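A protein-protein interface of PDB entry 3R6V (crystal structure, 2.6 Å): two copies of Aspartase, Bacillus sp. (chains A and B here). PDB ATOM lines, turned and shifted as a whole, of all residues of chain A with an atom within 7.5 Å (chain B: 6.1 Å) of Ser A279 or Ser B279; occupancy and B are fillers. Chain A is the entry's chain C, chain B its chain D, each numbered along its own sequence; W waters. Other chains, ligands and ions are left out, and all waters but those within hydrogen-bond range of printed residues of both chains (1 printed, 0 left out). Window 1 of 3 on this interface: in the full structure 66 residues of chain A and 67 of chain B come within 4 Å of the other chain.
The backbone carbonyl oxygen (O) of Asp A272 is in hydrogen-bond range of the side-chain hydroxyl (OG1) of Thr A275, 2.7 Å away.
The side-chain amino group of Lys A282 is in salt-bridge range of the side-chain carboxylate of Asp A344, 3.8 Å away.
The side-chain hydroxyl (OG) of Ser B278 is in hydrogen-bond range of the side-chain carboxylate (OD2) of Asp B344 (2.5 Å).
O of Asp A344 sits at hydrogen-bond distance from OG1 of Thr A348, 3.2 Å away.
OD2 of Asp A344 sits at hydrogen-bond distance from OG of Ser A278 (2.6 Å).
O of Thr A275 sits at hydrogen-bond distance from OG of Ser A279, 2.8 Å away.
Water W1 lies within hydrogen-bond range of OD2 of Asp A344 (2.9 Å), OG1 of Thr A348 (3.0 Å) and NZ of Lys B282 (3.2 Å).
The side-chain amino group (NZ) of Lys A282 lies within salt-bridge range of the side-chain carboxylate (OD1) of Asp B344.
OG of Ser A279 sits at hydrogen-bond distance from NZ of Lys B282 (3.4 Å).
The side-chain amino group (NZ) of Lys B282 sits close to the side-chain amino group (NZ) of Lys A282, 3.4 Å away.
NH1 of Arg A214 is in salt-bridge range of OE2 of Glu B276.
OG of Ser B279 is in hydrogen-bond range of NZ of Lys A282 (3.1 Å).
NZ of Lys B282 lies within salt-bridge range of OD1 of Asp A344.
Ser A279 touches its own counterpart, Ser B279.
Ser A279 touches Lys B282, and with the chains exchanged Lys A282 touches Ser B279.
Lys A282 touches its own counterpart, Lys B282.
Lys A282 touches Asp B344, and with the chains exchanged Asp A344 touches Lys B282.
12 positions are printed for both chains.
Of the 13 pairs that touch across the chains among the printed residues, 10 have their exchanged pair printed and touching as well.
Of the 12 printed residues of chain B, 6 touch a printed residue of chain A.
Hydrophobic or aromatic side chains of chain B within 4 Å of the printed part of chain A: Val B283.
Of the 22 printed residues of chain A, 8 touch a printed residue of chain B.
Printed residues of chain A that touch a printed residue of chain B: Arg A214, Thr A275, Ser A279, Lys A282, Val A283, Ile A286, Asp A344 and Thr A348.
Hydrophobic or aromatic side chains of chain A that line the printed part of chain B: Val A283 and Ile A286.
Among the printed residues, 13 pairs touch across the chains.
Ser A279 touches just these residues of chain B: Ser B279, Lys B282 and Val B283.
Of chain A, only Ser A279, Lys A282 and Val A283 come within 4 Å of Ser B279.
Printed residues of chain A within 4 Å of Glu B276: Arg A214.
Of the printed residues of chain B, Thr A275 touches Val B283.
Of the printed residues of chain A, Val B283 touches Thr A275 (3.7 Å) and Ser A279 (3.4 Å).
Of the printed residues of chain A, Lys B282 touches Ser A279, Lys A282, Asp A344 and Thr A348.
Of the printed residues of chain B, Ile A286 touches Thr B275.
The nearest printed residue of chain A that does not touch Glu B276 is Val A283 (4.05 Å).
CG1 of Val B283 touches OG1 of Thr A275, 3.7 Å away.
Ser A279 touches Ser B279.
CG2 of Val B283 touches OG of Ser A279, 3.4 Å away.
Val A283 touches Thr B275 (CG2 to OG1, 3.4 Å).
Val A283 touches Ser B279 (CG2 to OG, 3.5 Å).
CG2 of Thr B275 touches CD1 of Ile A286, at 3.7 Å.
CD of Lys B282 touches OG1 of Thr A348, at 3.4 Å.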
ATOM      1  N   ARG A 214     -11.531  28.847  17.692  1.00  0.00           N
ATOM      2  CA  ARG A 214     -10.649  29.328  18.769  1.00  0.00           C
ATOM      3  C   ARG A 214      -9.483  30.165  18.258  1.00  0.00           C
ATOM      4  O   ARG A 214      -9.155  31.193  18.845  1.00  0.00           O
ATOM      5  CB  ARG A 214     -10.099  28.172  19.602  1.00  0.00           C
ATOM      6  CG  ARG A 214     -11.126  27.432  20.397  1.00  0.00           C
ATOM      7  CD  ARG A 214     -10.480  26.333  21.210  1.00  0.00           C
ATOM      8  NE  ARG A 214     -10.116  25.146  20.425  1.00  0.00           N
ATOM      9  CZ  ARG A 214     -10.808  24.005  20.400  1.00  0.00           C
ATOM     10  NH1 ARG A 214     -11.924  23.880  21.111  1.00  0.00           N
ATOM     11  NH2 ARG A 214     -10.381  22.980  19.659  1.00  0.00           N
ATOM     12  N   ILE A 215      -8.848  29.717  17.182  1.00  0.00           N
ATOM     13  CA  ILE A 215      -7.729  30.460  16.593  1.00  0.00           C
ATOM     14  C   ILE A 215      -8.160  31.854  16.086  1.00  0.00           C
ATOM     15  O   ILE A 215      -7.489  32.852  16.354  1.00  0.00           O
ATOM     16  CB  ILE A 215      -7.015  29.644  15.484  1.00  0.00           C
ATOM     17  CG1 ILE A 215      -6.416  28.364  16.079  1.00  0.00           C
ATOM     18  CG2 ILE A 215      -5.909  30.462  14.849  1.00  0.00           C
ATOM     19  CD1 ILE A 215      -5.891  27.352  15.076  1.00  0.00           C
ATOM     20  N   THR A 218      -8.714  34.592  18.729  1.00  0.00           N
ATOM     21  CA  THR A 218      -7.528  35.142  19.388  1.00  0.00           C
ATOM     22  C   THR A 218      -7.009  36.398  18.699  1.00  0.00           C
ATOM     23  O   THR A 218      -6.141  37.081  19.226  1.00  0.00           O
ATOM     24  CB  THR A 218      -6.372  34.135  19.495  1.00  0.00           C
ATOM     25  OG1 THR A 218      -5.876  33.839  18.184  1.00  0.00           O
ATOM     26  CG2 THR A 218      -6.812  32.879  20.213  1.00  0.00           C
ATOM     27  N   ASP A 272      -0.485  38.873  27.680  1.00  0.00           N
ATOM     28  CA  ASP A 272      -1.500  37.821  27.653  1.00  0.00           C
ATOM     29  C   ASP A 272      -2.018  37.531  26.248  1.00  0.00           C
ATOM     30  O   ASP A 272      -2.271  36.370  25.917  1.00  0.00           O
ATOM     31  CB  ASP A 272      -2.659  38.106  28.614  1.00  0.00           C
ATOM     32  CG  ASP A 272      -3.336  39.428  28.340  1.00  0.00           C
ATOM     33  OD1 ASP A 272      -2.657  40.476  28.436  1.00  0.00           O
ATOM     34  OD2 ASP A 272      -4.552  39.421  28.044  1.00  0.00           O
ATOM     35  N   TYR A 274      -0.537  37.297  23.560  1.00  0.00           N
ATOM     36  CA  TYR A 274       0.351  36.377  22.842  1.00  0.00           C
ATOM     37  C   TYR A 274       0.207  34.932  23.330  1.00  0.00           C
ATOM     38  O   TYR A 274       0.270  33.986  22.536  1.00  0.00           O
ATOM     39  CB  TYR A 274       1.817  36.814  22.970  1.00  0.00           C
ATOM     40  CG  TYR A 274       2.097  38.254  22.606  1.00  0.00           C
ATOM     41  CD1 TYR A 274       2.550  39.152  23.568  1.00  0.00           C
ATOM     42  CD2 TYR A 274       1.918  38.722  21.302  1.00  0.00           C
ATOM     43  CE1 TYR A 274       2.818  40.476  23.250  1.00  0.00           C
ATOM     44  CE2 TYR A 274       2.183  40.052  20.969  1.00  0.00           C
ATOM     45  CZ  TYR A 274       2.631  40.923  21.951  1.00  0.00           C
ATOM     46  OH  TYR A 274       2.895  42.248  21.652  1.00  0.00           O
ATOM     47  N   THR A 275       0.026  34.767  24.634  1.00  0.00           N
ATOM     48  CA  THR A 275      -0.136  33.453  25.224  1.00  0.00           C
ATOM     49  C   THR A 275      -1.498  32.881  24.844  1.00  0.00           C
ATOM     50  O   THR A 275      -1.674  31.653  24.765  1.00  0.00           O
ATOM     51  CB  THR A 275      -0.003  33.509  26.746  1.00  0.00           C
ATOM     52  OG1 THR A 275      -0.703  34.653  27.248  1.00  0.00           O
ATOM     53  CG2 THR A 275       1.427  33.642  27.130  1.00  0.00           C
ATOM     54  N   GLU A 276      -2.457  33.780  24.618  1.00  0.00           N
ATOM     55  CA  GLU A 276      -3.773  33.407  24.112  1.00  0.00           C
ATOM     56  C   GLU A 276      -3.648  32.679  22.770  1.00  0.00           C
ATOM     57  O   GLU A 276      -4.183  31.599  22.608  1.00  0.00           O
ATOM     58  CB  GLU A 276      -4.653  34.640  23.981  1.00  0.00           C
ATOM     59  CG  GLU A 276      -6.109  34.349  23.717  1.00  0.00           C
ATOM     60  CD  GLU A 276      -6.967  35.603  23.737  1.00  0.00           C
ATOM     61  OE1 GLU A 276      -8.080  35.589  23.177  1.00  0.00           O
ATOM     62  OE2 GLU A 276      -6.533  36.612  24.315  1.00  0.00           O
ATOM     63  N   VAL A 277      -2.917  33.257  21.824  1.00  0.00           N
ATOM     64  CA  VAL A 277      -2.714  32.626  20.519  1.00  0.00           C
ATOM     65  C   VAL A 277      -2.047  31.245  20.639  1.00  0.00           C
ATOM     66  O   VAL A 277      -2.567  30.249  20.136  1.00  0.00           O
ATOM     67  CB  VAL A 277      -1.908  33.525  19.566  1.00  0.00           C
ATOM     68  CG1 VAL A 277      -1.768  32.858  18.203  1.00  0.00           C
ATOM     69  CG2 VAL A 277      -2.584  34.868  19.415  1.00  0.00           C
ATOM     70  N   SER A 278      -0.897  31.202  21.308  1.00  0.00           N
ATOM     71  CA  SER A 278      -0.148  29.967  21.491  1.00  0.00           C
ATOM     72  C   SER A 278      -1.025  28.844  22.041  1.00  0.00           C
ATOM     73  O   SER A 278      -1.006  27.741  21.520  1.00  0.00           O
ATOM     74  CB  SER A 278       1.073  30.212  22.390  1.00  0.00           C
ATOM     75  OG  SER A 278       1.874  29.044  22.498  1.00  0.00           O
ATOM     76  N   SER A 279      -1.795  29.143  23.083  1.00  0.00           N
ATOM     77  CA  SER A 279      -2.737  28.201  23.679  1.00  0.00           C
ATOM     78  C   SER A 279      -3.724  27.603  22.652  1.00  0.00           C
ATOM     79  O   SER A 279      -3.896  26.371  22.574  1.00  0.00           O
ATOM     80  CB  SER A 279      -3.494  28.884  24.818  1.00  0.00           C
ATOM     81  OG  SER A 279      -2.599  29.295  25.841  1.00  0.00           O
ATOM     82  N   ALA A 280      -4.352  28.471  21.859  1.00  0.00           N
ATOM     83  CA  ALA A 280      -5.246  28.031  20.796  1.00  0.00           C
ATOM     84  C   ALA A 280      -4.519  27.146  19.768  1.00  0.00           C
ATOM     85  O   ALA A 280      -5.063  26.122  19.319  1.00  0.00           O
ATOM     86  CB  ALA A 280      -5.922  29.222  20.128  1.00  0.00           C
ATOM     87  N   LEU A 281      -3.287  27.517  19.423  1.00  0.00           N
ATOM     88  CA  LEU A 281      -2.485  26.728  18.486  1.00  0.00           C
ATOM     89  C   LEU A 281      -2.060  25.383  19.083  1.00  0.00           C
ATOM     90  O   LEU A 281      -1.850  24.425  18.348  1.00  0.00           O
ATOM     91  CB  LEU A 281      -1.248  27.506  18.031  1.00  0.00           C
ATOM     92  CG  LEU A 281      -1.349  28.936  17.483  1.00  0.00           C
ATOM     93  CD1 LEU A 281       0.049  29.463  17.215  1.00  0.00           C
ATOM     94  CD2 LEU A 281      -2.211  29.015  16.238  1.00  0.00           C
ATOM     95  N   LYS A 282      -1.924  25.320  20.409  1.00  0.00           N
ATOM     96  CA  LYS A 282      -1.506  24.099  21.099  1.00  0.00           C
ATOM     97  C   LYS A 282      -2.661  23.122  21.061  1.00  0.00           C
ATOM     98  O   LYS A 282      -2.494  21.982  20.623  1.00  0.00           O
ATOM     99  CB  LYS A 282      -1.082  24.403  22.544  1.00  0.00           C
ATOM    100  CG  LYS A 282      -0.631  23.201  23.391  1.00  0.00           C
ATOM    101  CD  LYS A 282      -0.532  23.577  24.888  1.00  0.00           C
ATOM    102  CE  LYS A 282      -1.933  23.758  25.556  1.00  0.00           C
ATOM    103  NZ  LYS A 282      -1.989  24.647  26.804  1.00  0.00           N
ATOM    104  N   VAL A 283      -3.838  23.597  21.488  1.00  0.00           N
ATOM    105  CA  VAL A 283      -5.074  22.812  21.485  1.00  0.00           C
ATOM    106  C   VAL A 283      -5.305  22.216  20.109  1.00  0.00           C
ATOM    107  O   VAL A 283      -5.661  21.039  19.987  1.00  0.00           O
ATOM    108  CB  VAL A 283      -6.292  23.661  21.910  1.00  0.00           C
ATOM    109  CG1 VAL A 283      -7.589  22.946  21.589  1.00  0.00           C
ATOM    110  CG2 VAL A 283      -6.221  23.990  23.401  1.00  0.00           C
ATOM    111  N   CYS A 284      -5.080  23.021  19.073  1.00  0.00           N
ATOM    112  CA  CYS A 284      -5.226  22.555  17.694  1.00  0.00           C
ATOM    113  C   CYS A 284      -4.270  21.387  17.404  1.00  0.00           C
ATOM    114  O   CYS A 284      -4.708  20.333  16.945  1.00  0.00           O
ATOM    115  CB  CYS A 284      -5.032  23.699  16.697  1.00  0.00           C
ATOM    116  SG  CYS A 284      -5.163  23.194  14.967  1.00  0.00           S
ATOM    117  N   MET A 285      -2.982  21.558  17.702  1.00  0.00           N
ATOM    118  CA  MET A 285      -2.011  20.489  17.451  1.00  0.00           C
ATOM    119  C   MET A 285      -2.282  19.229  18.245  1.00  0.00           C
ATOM    120  O   MET A 285      -2.102  18.139  17.714  1.00  0.00           O
ATOM    121  CB  MET A 285      -0.574  20.948  17.653  1.00  0.00           C
ATOM    122  CG  MET A 285      -0.105  21.910  16.573  1.00  0.00           C
ATOM    123  SD  MET A 285      -0.746  21.553  14.913  1.00  0.00           S
ATOM    124  CE  MET A 285       0.166  20.062  14.471  1.00  0.00           C
ATOM    125  N   ILE A 286      -2.727  19.371  19.497  1.00  0.00           N
ATOM    126  CA  ILE A 286      -3.158  18.219  20.276  1.00  0.00           C
ATOM    127  C   ILE A 286      -4.115  17.372  19.433  1.00  0.00           C
ATOM    128  O   ILE A 286      -3.889  16.163  19.234  1.00  0.00           O
ATOM    129  CB  ILE A 286      -3.881  18.608  21.568  1.00  0.00           C
ATOM    130  CG1 ILE A 286      -2.989  19.462  22.465  1.00  0.00           C
ATOM    131  CG2 ILE A 286      -4.305  17.358  22.304  1.00  0.00           C
ATOM    132  CD1 ILE A 286      -3.648  19.881  23.788  1.00  0.00           C
ATOM    133  N   VAL A 340       5.121  22.477  18.461  1.00  0.00           N
ATOM    134  CA  VAL A 340       4.200  23.498  18.948  1.00  0.00           C
ATOM    135  C   VAL A 340       4.025  23.402  20.463  1.00  0.00           C
ATOM    136  O   VAL A 340       4.009  24.427  21.152  1.00  0.00           O
ATOM    137  CB  VAL A 340       2.840  23.452  18.217  1.00  0.00           C
ATOM    138  CG1 VAL A 340       1.874  24.417  18.840  1.00  0.00           C
ATOM    139  CG2 VAL A 340       3.035  23.814  16.759  1.00  0.00           C
ATOM    140  N   ASP A 344       5.027  26.282  23.075  1.00  0.00           N
ATOM    141  CA  ASP A 344       4.053  26.838  23.988  1.00  0.00           C
ATOM    142  C   ASP A 344       4.655  27.027  25.381  1.00  0.00           C
ATOM    143  O   ASP A 344       4.411  28.054  26.025  1.00  0.00           O
ATOM    144  CB  ASP A 344       2.784  25.992  24.045  1.00  0.00           C
ATOM    145  CG  ASP A 344       1.715  26.612  24.923  1.00  0.00           C
ATOM    146  OD1 ASP A 344       1.402  26.027  25.983  1.00  0.00           O
ATOM    147  OD2 ASP A 344       1.205  27.697  24.567  1.00  0.00           O
ATOM    148  N   ILE A 347       6.997  30.032  25.399  1.00  0.00           N
ATOM    149  CA  ILE A 347       6.150  31.206  25.436  1.00  0.00           C
ATOM    150  C   ILE A 347       5.535  31.395  26.837  1.00  0.00           C
ATOM    151  O   ILE A 347       5.476  32.520  27.350  1.00  0.00           O
ATOM    152  CB  ILE A 347       5.050  31.080  24.376  1.00  0.00           C
ATOM    153  CG1 ILE A 347       5.679  31.144  22.984  1.00  0.00           C
ATOM    154  CG2 ILE A 347       3.967  32.152  24.562  1.00  0.00           C
ATOM    155  CD1 ILE A 347       4.733  30.829  21.863  1.00  0.00           C
ATOM    156  N   THR A 348       5.086  30.308  27.465  1.00  0.00           N
ATOM    157  CA  THR A 348       4.545  30.408  28.827  1.00  0.00           C
ATOM    158  C   THR A 348       5.591  30.979  29.783  1.00  0.00           C
ATOM    159  O   THR A 348       5.294  31.887  30.541  1.00  0.00           O
ATOM    160  CB  THR A 348       4.003  29.050  29.346  1.00  0.00           C
ATOM    161  OG1 THR A 348       2.777  28.735  28.669  1.00  0.00           O
ATOM    162  CG2 THR A 348       3.731  29.114  30.832  1.00  0.00           C
ATOM    163  N   LEU A 369       6.105  31.902  18.791  1.00  0.00           N
ATOM    164  CA  LEU A 369       4.739  32.109  18.319  1.00  0.00           C
ATOM    165  C   LEU A 369       4.671  32.236  16.781  1.00  0.00           C
ATOM    166  O   LEU A 369       3.829  31.593  16.144  1.00  0.00           O
ATOM    167  CB  LEU A 369       4.129  33.330  19.001  1.00  0.00           C
ATOM    168  CG  LEU A 369       2.692  33.721  18.669  1.00  0.00           C
ATOM    169  CD1 LEU A 369       1.727  32.763  19.303  1.00  0.00           C
ATOM    170  CD2 LEU A 369       2.440  35.127  19.153  1.00  0.00           C
ATOM    171  N   TYR B 274     -11.698  20.235  27.006  1.00  0.00           N
ATOM    172  CA  TYR B 274     -10.994  20.287  28.295  1.00  0.00           C
ATOM    173  C   TYR B 274      -9.674  21.062  28.230  1.00  0.00           C
ATOM    174  O   TYR B 274      -9.375  21.862  29.111  1.00  0.00           O
ATOM    175  CB  TYR B 274     -10.761  18.886  28.856  1.00  0.00           C
ATOM    176  CG  TYR B 274     -11.989  18.016  28.848  1.00  0.00           C
ATOM    177  CD1 TYR B 274     -12.033  16.852  28.086  1.00  0.00           C
ATOM    178  CD2 TYR B 274     -13.115  18.352  29.604  1.00  0.00           C
ATOM    179  CE1 TYR B 274     -13.170  16.041  28.070  1.00  0.00           C
ATOM    180  CE2 TYR B 274     -14.251  17.550  29.596  1.00  0.00           C
ATOM    181  CZ  TYR B 274     -14.270  16.400  28.826  1.00  0.00           C
ATOM    182  OH  TYR B 274     -15.386  15.601  28.822  1.00  0.00           O
ATOM    183  N   THR B 275      -8.893  20.821  27.191  1.00  0.00           N
ATOM    184  CA  THR B 275      -7.661  21.557  26.972  1.00  0.00           C
ATOM    185  C   THR B 275      -7.951  23.039  26.711  1.00  0.00           C
ATOM    186  O   THR B 275      -7.129  23.908  27.027  1.00  0.00           O
ATOM    187  CB  THR B 275      -6.857  20.974  25.797  1.00  0.00           C
ATOM    188  OG1 THR B 275      -7.618  21.095  24.585  1.00  0.00           O
ATOM    189  CG2 THR B 275      -6.565  19.514  26.037  1.00  0.00           C
ATOM    190  N   GLU B 276      -9.122  23.320  26.146  1.00  0.00           N
ATOM    191  CA  GLU B 276      -9.567  24.700  25.978  1.00  0.00           C
ATOM    192  C   GLU B 276      -9.726  25.380  27.340  1.00  0.00           C
ATOM    193  O   GLU B 276      -9.229  26.497  27.533  1.00  0.00           O
ATOM    194  CB  GLU B 276     -10.867  24.785  25.179  1.00  0.00           C
ATOM    195  CG  GLU B 276     -11.229  26.185  24.741  1.00  0.00           C
ATOM    196  CD  GLU B 276     -12.610  26.274  24.087  1.00  0.00           C
ATOM    197  OE1 GLU B 276     -13.261  27.331  24.249  1.00  0.00           O
ATOM    198  OE2 GLU B 276     -13.046  25.301  23.419  1.00  0.00           O
ATOM    199  N   VAL B 277     -10.396  24.721  28.285  1.00  0.00           N
ATOM    200  CA  VAL B 277     -10.503  25.285  29.637  1.00  0.00           C
ATOM    201  C   VAL B 277      -9.135  25.428  30.302  1.00  0.00           C
ATOM    202  O   VAL B 277      -8.835  26.470  30.865  1.00  0.00           O
ATOM    203  CB  VAL B 277     -11.469  24.477  30.536  1.00  0.00           C
ATOM    204  CG1 VAL B 277     -11.496  25.037  31.967  1.00  0.00           C
ATOM    205  CG2 VAL B 277     -12.870  24.495  29.939  1.00  0.00           C
ATOM    206  N   SER B 278      -8.309  24.386  30.208  1.00  0.00           N
ATOM    207  CA  SER B 278      -6.958  24.373  30.797  1.00  0.00           C
ATOM    208  C   SER B 278      -6.093  25.531  30.307  1.00  0.00           C
ATOM    209  O   SER B 278      -5.450  26.228  31.096  1.00  0.00           O
ATOM    210  CB  SER B 278      -6.253  23.054  30.468  1.00  0.00           C
ATOM    211  OG  SER B 278      -4.995  22.966  31.115  1.00  0.00           O
ATOM    212  N   SER B 279      -6.088  25.722  28.992  1.00  0.00           N
ATOM    213  CA  SER B 279      -5.285  26.756  28.357  1.00  0.00           C
ATOM    214  C   SER B 279      -5.656  28.131  28.885  1.00  0.00           C
ATOM    215  O   SER B 279      -4.780  28.951  29.167  1.00  0.00           O
ATOM    216  CB  SER B 279      -5.448  26.693  26.839  1.00  0.00           C
ATOM    217  OG  SER B 279      -4.983  25.441  26.374  1.00  0.00           O
ATOM    218  N   ALA B 280      -6.949  28.370  29.046  1.00  0.00           N
ATOM    219  CA  ALA B 280      -7.406  29.654  29.531  1.00  0.00           C
ATOM    220  C   ALA B 280      -7.014  29.847  31.000  1.00  0.00           C
ATOM    221  O   ALA B 280      -6.624  30.962  31.387  1.00  0.00           O
ATOM    222  CB  ALA B 280      -8.887  29.808  29.324  1.00  0.00           C
ATOM    223  N   LEU B 281      -7.100  28.776  31.801  1.00  0.00           N
ATOM    224  CA  LEU B 281      -6.614  28.811  33.195  1.00  0.00           C
ATOM    225  C   LEU B 281      -5.120  29.113  33.297  1.00  0.00           C
ATOM    226  O   LEU B 281      -4.704  29.932  34.120  1.00  0.00           O
ATOM    227  CB  LEU B 281      -6.930  27.515  33.956  1.00  0.00           C
ATOM    228  CG  LEU B 281      -8.393  27.048  34.017  1.00  0.00           C
ATOM    229  CD1 LEU B 281      -8.504  25.727  34.757  1.00  0.00           C
ATOM    230  CD2 LEU B 281      -9.347  28.094  34.600  1.00  0.00           C
ATOM    231  N   LYS B 282      -4.326  28.452  32.452  1.00  0.00           N
ATOM    232  CA  LYS B 282      -2.870  28.622  32.416  1.00  0.00           C
ATOM    233  C   LYS B 282      -2.489  30.063  32.090  1.00  0.00           C
ATOM    234  O   LYS B 282      -1.630  30.649  32.751  1.00  0.00           O
ATOM    235  CB  LYS B 282      -2.248  27.640  31.418  1.00  0.00           C
ATOM    236  CG  LYS B 282      -0.715  27.666  31.312  1.00  0.00           C
ATOM    237  CD  LYS B 282      -0.267  28.136  29.935  1.00  0.00           C
ATOM    238  CE  LYS B 282      -0.153  26.994  28.926  1.00  0.00           C
ATOM    239  NZ  LYS B 282      -0.301  27.466  27.482  1.00  0.00           N
ATOM    240  N   VAL B 283      -3.154  30.638  31.094  1.00  0.00           N
ATOM    241  CA  VAL B 283      -2.909  32.026  30.695  1.00  0.00           C
ATOM    242  C   VAL B 283      -3.209  32.996  31.837  1.00  0.00           C
ATOM    243  O   VAL B 283      -2.502  33.981  32.035  1.00  0.00           O
ATOM    244  CB  VAL B 283      -3.729  32.400  29.436  1.00  0.00           C
ATOM    245  CG1 VAL B 283      -3.745  33.926  29.205  1.00  0.00           C
ATOM    246  CG2 VAL B 283      -3.184  31.666  28.214  1.00  0.00           C
ATOM    247  N   CYS B 284      -4.258  32.701  32.589  1.00  0.00           N
ATOM    248  CA  CYS B 284      -4.626  33.509  33.735  1.00  0.00           C
ATOM    249  C   CYS B 284      -3.542  33.459  34.809  1.00  0.00           C
ATOM    250  O   CYS B 284      -3.163  34.481  35.361  1.00  0.00           O
ATOM    251  CB  CYS B 284      -5.962  33.044  34.307  1.00  0.00           C
ATOM    252  SG  CYS B 284      -6.470  33.963  35.766  1.00  0.00           S
ATOM    253  N   ASP B 344      -1.421  21.639  33.300  1.00  0.00           N
ATOM    254  CA  ASP B 344      -1.740  21.878  31.903  1.00  0.00           C
ATOM    255  C   ASP B 344      -0.964  20.985  30.938  1.00  0.00           C
ATOM    256  O   ASP B 344      -1.456  20.674  29.853  1.00  0.00           O
ATOM    257  CB  ASP B 344      -1.579  23.348  31.515  1.00  0.00           C
ATOM    258  CG  ASP B 344      -1.851  23.574  30.041  1.00  0.00           C
ATOM    259  OD1 ASP B 344      -0.886  23.670  29.253  1.00  0.00           O
ATOM    260  OD2 ASP B 344      -3.045  23.588  29.658  1.00  0.00           O
HETATM  261  O   HOH W   1       1.301  30.005  26.394  1.00  0.00           O
